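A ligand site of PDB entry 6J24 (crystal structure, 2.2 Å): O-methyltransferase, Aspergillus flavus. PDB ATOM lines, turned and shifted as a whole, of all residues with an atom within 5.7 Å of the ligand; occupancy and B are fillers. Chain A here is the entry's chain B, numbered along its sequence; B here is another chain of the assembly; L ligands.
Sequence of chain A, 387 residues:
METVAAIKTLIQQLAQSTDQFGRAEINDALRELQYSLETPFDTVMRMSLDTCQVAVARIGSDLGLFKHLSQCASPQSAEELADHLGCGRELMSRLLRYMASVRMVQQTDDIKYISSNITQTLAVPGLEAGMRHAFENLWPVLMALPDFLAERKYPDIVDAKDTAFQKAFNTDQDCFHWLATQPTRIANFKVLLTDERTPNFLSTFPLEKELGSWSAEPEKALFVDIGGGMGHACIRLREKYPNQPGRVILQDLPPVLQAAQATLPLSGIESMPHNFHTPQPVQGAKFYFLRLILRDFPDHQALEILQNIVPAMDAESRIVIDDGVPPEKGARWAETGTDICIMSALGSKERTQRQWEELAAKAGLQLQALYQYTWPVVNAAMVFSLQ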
ATOM      1  N   GLY A 130      21.134  18.278  26.752  1.00  0.00           N
ATOM      2  CA  GLY A 130      21.139  18.898  25.436  1.00  0.00           C
ATOM      3  C   GLY A 130      22.376  18.530  24.639  1.00  0.00           C
ATOM      4  O   GLY A 130      22.306  18.270  23.435  1.00  0.00           O
ATOM      5  N   HIS A 133      21.940  14.854  23.645  1.00  0.00           N
ATOM      6  CA  HIS A 133      21.029  14.884  22.498  1.00  0.00           C
ATOM      7  C   HIS A 133      21.776  15.201  21.209  1.00  0.00           C
ATOM      8  O   HIS A 133      21.588  14.539  20.180  1.00  0.00           O
ATOM      9  CB  HIS A 133      19.929  15.907  22.771  1.00  0.00           C
ATOM     10  CG  HIS A 133      19.030  16.150  21.605  1.00  0.00           C
ATOM     11  ND1 HIS A 133      18.181  15.195  21.097  1.00  0.00           N
ATOM     12  CD2 HIS A 133      18.820  17.270  20.863  1.00  0.00           C
ATOM     13  CE1 HIS A 133      17.494  15.693  20.091  1.00  0.00           C
ATOM     14  NE2 HIS A 133      17.859  16.956  19.924  1.00  0.00           N
ATOM     15  N   ASN A 137      21.655  12.098  18.694  1.00  0.00           N
ATOM     16  CA  ASN A 137      20.533  12.257  17.768  1.00  0.00           C
ATOM     17  C   ASN A 137      20.821  13.220  16.628  1.00  0.00           C
ATOM     18  O   ASN A 137      20.388  12.976  15.506  1.00  0.00           O
ATOM     19  CB  ASN A 137      19.286  12.731  18.520  1.00  0.00           C
ATOM     20  CG  ASN A 137      18.851  11.756  19.591  1.00  0.00           C
ATOM     21  OD1 ASN A 137      18.932  10.536  19.410  1.00  0.00           O
ATOM     22  ND2 ASN A 137      18.394  12.279  20.723  1.00  0.00           N
ATOM     23  N   LEU A 138      21.529  14.325  16.890  1.00  0.00           N
ATOM     24  CA  LEU A 138      21.774  15.312  15.843  1.00  0.00           C
ATOM     25  C   LEU A 138      22.897  14.880  14.909  1.00  0.00           C
ATOM     26  O   LEU A 138      22.756  14.941  13.682  1.00  0.00           O
ATOM     27  CB  LEU A 138      22.110  16.661  16.481  1.00  0.00           C
ATOM     28  CG  LEU A 138      21.166  17.782  16.083  1.00  0.00           C
ATOM     29  CD1 LEU A 138      21.000  17.720  14.570  1.00  0.00           C
ATOM     30  CD2 LEU A 138      19.841  17.619  16.800  1.00  0.00           C
ATOM     31  N   CYS A 175      10.835  10.744  13.170  1.00  0.00           N
ATOM     32  CA  CYS A 175      11.671  10.836  14.368  1.00  0.00           C
ATOM     33  C   CYS A 175      10.858  10.616  15.644  1.00  0.00           C
ATOM     34  O   CYS A 175      11.315   9.930  16.565  1.00  0.00           O
ATOM     35  CB  CYS A 175      12.371  12.189  14.403  1.00  0.00           C
ATOM     36  SG  CYS A 175      13.315  12.498  15.911  1.00  0.00           S
ATOM     37  N   PHE A 176       9.666  11.201  15.710  1.00  0.00           N
ATOM     38  CA  PHE A 176       8.904  11.134  16.950  1.00  0.00           C
ATOM     39  C   PHE A 176       8.510   9.697  17.282  1.00  0.00           C
ATOM     40  O   PHE A 176       8.749   9.223  18.395  1.00  0.00           O
ATOM     41  CB  PHE A 176       7.669  12.043  16.856  1.00  0.00           C
ATOM     42  CG  PHE A 176       8.015  13.495  16.703  1.00  0.00           C
ATOM     43  CD1 PHE A 176       8.723  14.156  17.697  1.00  0.00           C
ATOM     44  CD2 PHE A 176       7.637  14.203  15.577  1.00  0.00           C
ATOM     45  CE1 PHE A 176       9.050  15.494  17.583  1.00  0.00           C
ATOM     46  CE2 PHE A 176       7.951  15.547  15.449  1.00  0.00           C
ATOM     47  CZ  PHE A 176       8.666  16.193  16.445  1.00  0.00           C
ATOM     48  N   PHE A 189      15.753  12.408  26.680  1.00  0.00           N
ATOM     49  CA  PHE A 189      14.727  13.379  26.279  1.00  0.00           C
ATOM     50  C   PHE A 189      13.914  13.831  27.478  1.00  0.00           C
ATOM     51  O   PHE A 189      13.512  14.998  27.560  1.00  0.00           O
ATOM     52  CB  PHE A 189      13.821  12.759  25.213  1.00  0.00           C
ATOM     53  CG  PHE A 189      12.867  13.741  24.579  1.00  0.00           C
ATOM     54  CD1 PHE A 189      13.225  14.425  23.423  1.00  0.00           C
ATOM     55  CD2 PHE A 189      11.613  13.974  25.132  1.00  0.00           C
ATOM     56  CE1 PHE A 189      12.348  15.330  22.827  1.00  0.00           C
ATOM     57  CE2 PHE A 189      10.732  14.884  24.556  1.00  0.00           C
ATOM     58  CZ  PHE A 189      11.102  15.561  23.401  1.00  0.00           C
ATOM     59  N   LEU A 192      15.821  16.448  29.213  1.00  0.00           N
ATOM     60  CA  LEU A 192      15.843  17.668  28.415  1.00  0.00           C
ATOM     61  C   LEU A 192      14.632  18.548  28.698  1.00  0.00           C
ATOM     62  O   LEU A 192      14.738  19.778  28.726  1.00  0.00           O
ATOM     63  CB  LEU A 192      15.932  17.304  26.934  1.00  0.00           C
ATOM     64  CG  LEU A 192      16.401  18.376  25.960  1.00  0.00           C
ATOM     65  CD1 LEU A 192      17.680  19.001  26.472  1.00  0.00           C
ATOM     66  CD2 LEU A 192      16.638  17.737  24.608  1.00  0.00           C
ATOM     67  N   ARG A 197      14.144  27.441  29.616  1.00  0.00           N
ATOM     68  CA  ARG A 197      14.827  28.551  28.976  1.00  0.00           C
ATOM     69  C   ARG A 197      14.505  29.860  29.688  1.00  0.00           C
ATOM     70  O   ARG A 197      13.402  30.055  30.200  1.00  0.00           O
ATOM     71  CB  ARG A 197      14.415  28.643  27.513  1.00  0.00           C
ATOM     72  CG  ARG A 197      14.898  27.478  26.645  1.00  0.00           C
ATOM     73  CD  ARG A 197      14.886  27.892  25.183  1.00  0.00           C
ATOM     74  NE  ARG A 197      15.084  26.787  24.262  1.00  0.00           N
ATOM     75  CZ  ARG A 197      15.122  26.928  22.934  1.00  0.00           C
ATOM     76  NH1 ARG A 197      15.308  25.858  22.153  1.00  0.00           N
ATOM     77  NH2 ARG A 197      14.975  28.126  22.381  1.00  0.00           N
ATOM     78  N   ARG A 295       7.507  24.727  15.112  1.00  0.00           N
ATOM     79  CA  ARG A 295       8.823  24.600  14.476  1.00  0.00           C
ATOM     80  C   ARG A 295       9.187  23.150  14.179  1.00  0.00           C
ATOM     81  O   ARG A 295       9.991  22.902  13.275  1.00  0.00           O
ATOM     82  CB  ARG A 295       9.905  25.211  15.362  1.00  0.00           C
ATOM     83  CG  ARG A 295      10.270  24.329  16.539  1.00  0.00           C
ATOM     84  CD  ARG A 295      11.134  25.017  17.558  1.00  0.00           C
ATOM     85  NE  ARG A 295      12.516  25.121  17.134  1.00  0.00           N
ATOM     86  CZ  ARG A 295      13.078  26.247  16.712  1.00  0.00           C
ATOM     87  NH1 ARG A 295      14.348  26.246  16.318  1.00  0.00           N
ATOM     88  NH2 ARG A 295      12.376  27.370  16.679  1.00  0.00           N
ATOM     89  N   ASP A 296       8.620  22.193  14.921  1.00  0.00           N
ATOM     90  CA  ASP A 296       9.008  20.795  14.795  1.00  0.00           C
ATOM     91  C   ASP A 296       8.231  20.048  13.712  1.00  0.00           C
ATOM     92  O   ASP A 296       8.419  18.827  13.576  1.00  0.00           O
ATOM     93  CB  ASP A 296       8.842  20.087  16.135  1.00  0.00           C
ATOM     94  CG  ASP A 296      10.017  20.319  17.068  1.00  0.00           C
ATOM     95  OD1 ASP A 296      10.939  21.070  16.694  1.00  0.00           O
ATOM     96  OD2 ASP A 296      10.031  19.746  18.174  1.00  0.00           O
ATOM     97  N   THR A 338      19.727  25.762  13.667  1.00  0.00           N
ATOM     98  CA  THR A 338      18.553  24.990  14.064  1.00  0.00           C
ATOM     99  C   THR A 338      17.730  24.619  12.846  1.00  0.00           C
ATOM    100  O   THR A 338      17.246  23.490  12.738  1.00  0.00           O
ATOM    101  CB  THR A 338      17.694  25.765  15.077  1.00  0.00           C
ATOM    102  OG1 THR A 338      17.248  27.001  14.515  1.00  0.00           O
ATOM    103  CG2 THR A 338      18.458  26.038  16.349  1.00  0.00           C
ATOM    104  N   CYS A 341      19.143  21.605  11.186  1.00  0.00           N
ATOM    105  CA  CYS A 341      19.010  20.394  11.990  1.00  0.00           C
ATOM    106  C   CYS A 341      17.597  19.832  11.942  1.00  0.00           C
ATOM    107  O   CYS A 341      17.410  18.617  11.825  1.00  0.00           O
ATOM    108  CB  CYS A 341      19.401  20.677  13.438  1.00  0.00           C
ATOM    109  SG  CYS A 341      21.154  20.996  13.665  1.00  0.00           S
ATOM    110  N   ILE A 342      16.587  20.702  12.080  1.00  0.00           N
ATOM    111  CA  ILE A 342      15.202  20.212  12.081  1.00  0.00           C
ATOM    112  C   ILE A 342      14.780  19.823  10.672  1.00  0.00           C
ATOM    113  O   ILE A 342      13.927  18.944  10.499  1.00  0.00           O
ATOM    114  CB  ILE A 342      14.238  21.239  12.702  1.00  0.00           C
ATOM    115  CG1 ILE A 342      14.166  22.522  11.846  1.00  0.00           C
ATOM    116  CG2 ILE A 342      14.632  21.555  14.147  1.00  0.00           C
ATOM    117  CD1 ILE A 342      13.341  23.629  12.460  1.00  0.00           C
ATOM    118  N   ALA A 345      16.267  16.265  10.475  1.00  0.00           N
ATOM    119  CA  ALA A 345      15.731  15.287  11.409  1.00  0.00           C
ATOM    120  C   ALA A 345      14.210  15.216  11.389  1.00  0.00           C
ATOM    121  O   ALA A 345      13.648  14.119  11.553  1.00  0.00           O
ATOM    122  CB  ALA A 345      16.205  15.600  12.835  1.00  0.00           C
ATOM    123  N   LEU A 346      13.520  16.334  11.171  1.00  0.00           N
ATOM    124  CA  LEU A 346      12.075  16.401  11.328  1.00  0.00           C
ATOM    125  C   LEU A 346      11.349  16.834  10.059  1.00  0.00           C
ATOM    126  O   LEU A 346      10.114  16.826  10.048  1.00  0.00           O
ATOM    127  CB  LEU A 346      11.697  17.369  12.455  1.00  0.00           C
ATOM    128  CG  LEU A 346      12.431  17.208  13.779  1.00  0.00           C
ATOM    129  CD1 LEU A 346      12.055  18.331  14.743  1.00  0.00           C
ATOM    130  CD2 LEU A 346      12.122  15.856  14.383  1.00  0.00           C
ATOM    131  N   PHE B  41      23.117  28.240  28.181  1.00  0.00           N
ATOM    132  CA  PHE B  41      22.354  27.791  27.015  1.00  0.00           C
ATOM    133  C   PHE B  41      23.125  28.023  25.725  1.00  0.00           C
ATOM    134  O   PHE B  41      23.045  27.225  24.794  1.00  0.00           O
ATOM    135  CB  PHE B  41      21.020  28.522  26.991  1.00  0.00           C
ATOM    136  CG  PHE B  41      20.165  28.207  25.798  1.00  0.00           C
ATOM    137  CD1 PHE B  41      19.555  26.977  25.677  1.00  0.00           C
ATOM    138  CD2 PHE B  41      19.957  29.170  24.813  1.00  0.00           C
ATOM    139  CE1 PHE B  41      18.762  26.696  24.584  1.00  0.00           C
ATOM    140  CE2 PHE B  41      19.170  28.884  23.713  1.00  0.00           C
ATOM    141  CZ  PHE B  41      18.566  27.651  23.599  1.00  0.00           C
ATOM    142  N   VAL B  44      25.681  25.117  25.175  1.00  0.00           N
ATOM    143  CA  VAL B  44      25.108  23.896  24.610  1.00  0.00           C
ATOM    144  C   VAL B  44      24.716  24.118  23.156  1.00  0.00           C
ATOM    145  O   VAL B  44      24.929  23.257  22.300  1.00  0.00           O
ATOM    146  CB  VAL B  44      23.898  23.418  25.440  1.00  0.00           C
ATOM    147  CG1 VAL B  44      23.260  22.200  24.764  1.00  0.00           C
ATOM    148  CG2 VAL B  44      24.324  23.115  26.870  1.00  0.00           C
ATOM    149  N   MET B  45      24.141  25.288  22.870  1.00  0.00           N
ATOM    150  CA  MET B  45      23.741  25.619  21.514  1.00  0.00           C
ATOM    151  C   MET B  45      24.954  25.637  20.581  1.00  0.00           C
ATOM    152  O   MET B  45      24.903  25.095  19.477  1.00  0.00           O
ATOM    153  CB  MET B  45      23.014  26.960  21.513  1.00  0.00           C
ATOM    154  CG  MET B  45      22.013  27.198  20.382  1.00  0.00           C
ATOM    155  SD  MET B  45      20.550  26.127  20.329  1.00  0.00           S
ATOM    156  CE  MET B  45      20.470  25.436  21.968  1.00  0.00           C
ATOM    157  N   SER B  48      26.100  22.120  19.872  1.00  0.00           N
ATOM    158  CA  SER B  48      25.156  21.395  19.024  1.00  0.00           C
ATOM    159  C   SER B  48      25.276  21.823  17.561  1.00  0.00           C
ATOM    160  O   SER B  48      25.219  20.979  16.660  1.00  0.00           O
ATOM    161  CB  SER B  48      23.726  21.609  19.516  1.00  0.00           C
ATOM    162  OG  SER B  48      23.601  21.338  20.895  1.00  0.00           O
ATOM    163  N   LEU B  49      25.453  23.131  17.315  1.00  0.00           N
ATOM    164  CA  LEU B  49      25.289  23.635  15.947  1.00  0.00           C
ATOM    165  C   LEU B  49      26.593  23.816  15.172  1.00  0.00           C
ATOM    166  O   LEU B  49      26.565  23.750  13.943  1.00  0.00           O
ATOM    167  CB  LEU B  49      24.536  24.960  15.977  1.00  0.00           C
ATOM    168  CG  LEU B  49      23.133  24.916  16.603  1.00  0.00           C
ATOM    169  CD1 LEU B  49      22.463  26.270  16.499  1.00  0.00           C
ATOM    170  CD2 LEU B  49      22.256  23.834  15.965  1.00  0.00           C
HETATM  171  C1  LIG L   1      17.175  21.796  17.223  1.00  0.00           C
HETATM  172  C2  LIG L   1      18.162  22.774  17.430  1.00  0.00           C
HETATM  173  C3  LIG L   1      19.208  22.269  18.517  1.00  0.00           C
HETATM  174  C4  LIG L   1      18.547  22.371  19.823  1.00  0.00           C
HETATM  175  C5  LIG L   1      19.455  21.597  20.805  1.00  0.00           C
HETATM  176  C6  LIG L   1      18.954  21.647  22.284  1.00  0.00           C
HETATM  177  C7  LIG L   1      17.344  21.716  22.308  1.00  0.00           C
HETATM  178  C8  LIG L   1      16.719  21.069  21.059  1.00  0.00           C
HETATM  179  C9  LIG L   1      16.927  21.971  19.794  1.00  0.00           C
HETATM  180  C10 LIG L   1      16.407  21.320  18.647  1.00  0.00           C
HETATM  181  C11 LIG L   1      16.276  19.885  18.438  1.00  0.00           C
HETATM  182  C12 LIG L   1      15.113  19.275  17.855  1.00  0.00           C
HETATM  183  C13 LIG L   1      13.795  19.908  18.186  1.00  0.00           C
HETATM  184  C14 LIG L   1      15.082  22.124  18.289  1.00  0.00           C
HETATM  185  C15 LIG L   1      15.270  17.812  17.584  1.00  0.00           C
HETATM  186  C16 LIG L   1      14.457  16.884  18.209  1.00  0.00           C
HETATM  187  C17 LIG L   1      14.633  15.549  17.933  1.00  0.00           C
HETATM  188  C18 LIG L   1      15.630  15.167  17.080  1.00  0.00           C
HETATM  189  C19 LIG L   1      16.450  16.106  16.482  1.00  0.00           C
HETATM  190  C20 LIG L   1      16.273  17.440  16.744  1.00  0.00           C
HETATM  191  C21 LIG L   1      18.060  20.734  16.702  1.00  0.00           C
HETATM  192  C22 LIG L   1      15.265  20.806  21.351  1.00  0.00           C
HETATM  193  N1  LIG L   1      13.806  21.379  18.078  1.00  0.00           N
HETATM  194  O1  LIG L   1      17.164  19.221  18.744  1.00  0.00           O
HETATM  195  O2  LIG L   1      15.062  23.284  18.173  1.00  0.00           O
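A ring nitrogen (NE2) of His 133 sits at hydrogen-bond distance from an oxygen (O1) of the ligand, at 2.6 Å. A nitrogen (N1) of the ligand is in hydrogen-bond range of the side-chain carboxylate (OD1) of Asp 296. An oxygen (O2) of the ligand is in hydrogen-bond range of the guanidinium group of Arg 295 (3.3 Å).
The backbone carbonyl oxygen (O) of His 133 lies within hydrogen-bond range of the backbone NH (N) of Leu 138, at 3.3 Å. A ring nitrogen (ND1) of His 133 sits at hydrogen-bond distance from the side-chain amide nitrogen of Asn 137, at 2.9 Å. The guanidinium group of Arg 295 is in hydrogen-bond range of the side-chain hydroxyl of Thr 338 (3.5 Å).
Residues that only touch the ligand: Thr 338, Cys 341, Leu 138, Ala 345, Cys 175 and Ile 342. Hydrophobic or aromatic side chains within 4 Å of the ligand: His 133, Leu 138, Ile 342 and Ala 345. Within 4 Å of the ligand: His 133, Leu 138, Cys 175, Arg 295, Asp 296, Thr 338, Cys 341, Ile 342 and Ala 345. The nearest printed residue that does not touch the ligand is Met 45 of chain B (4.1 Å).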
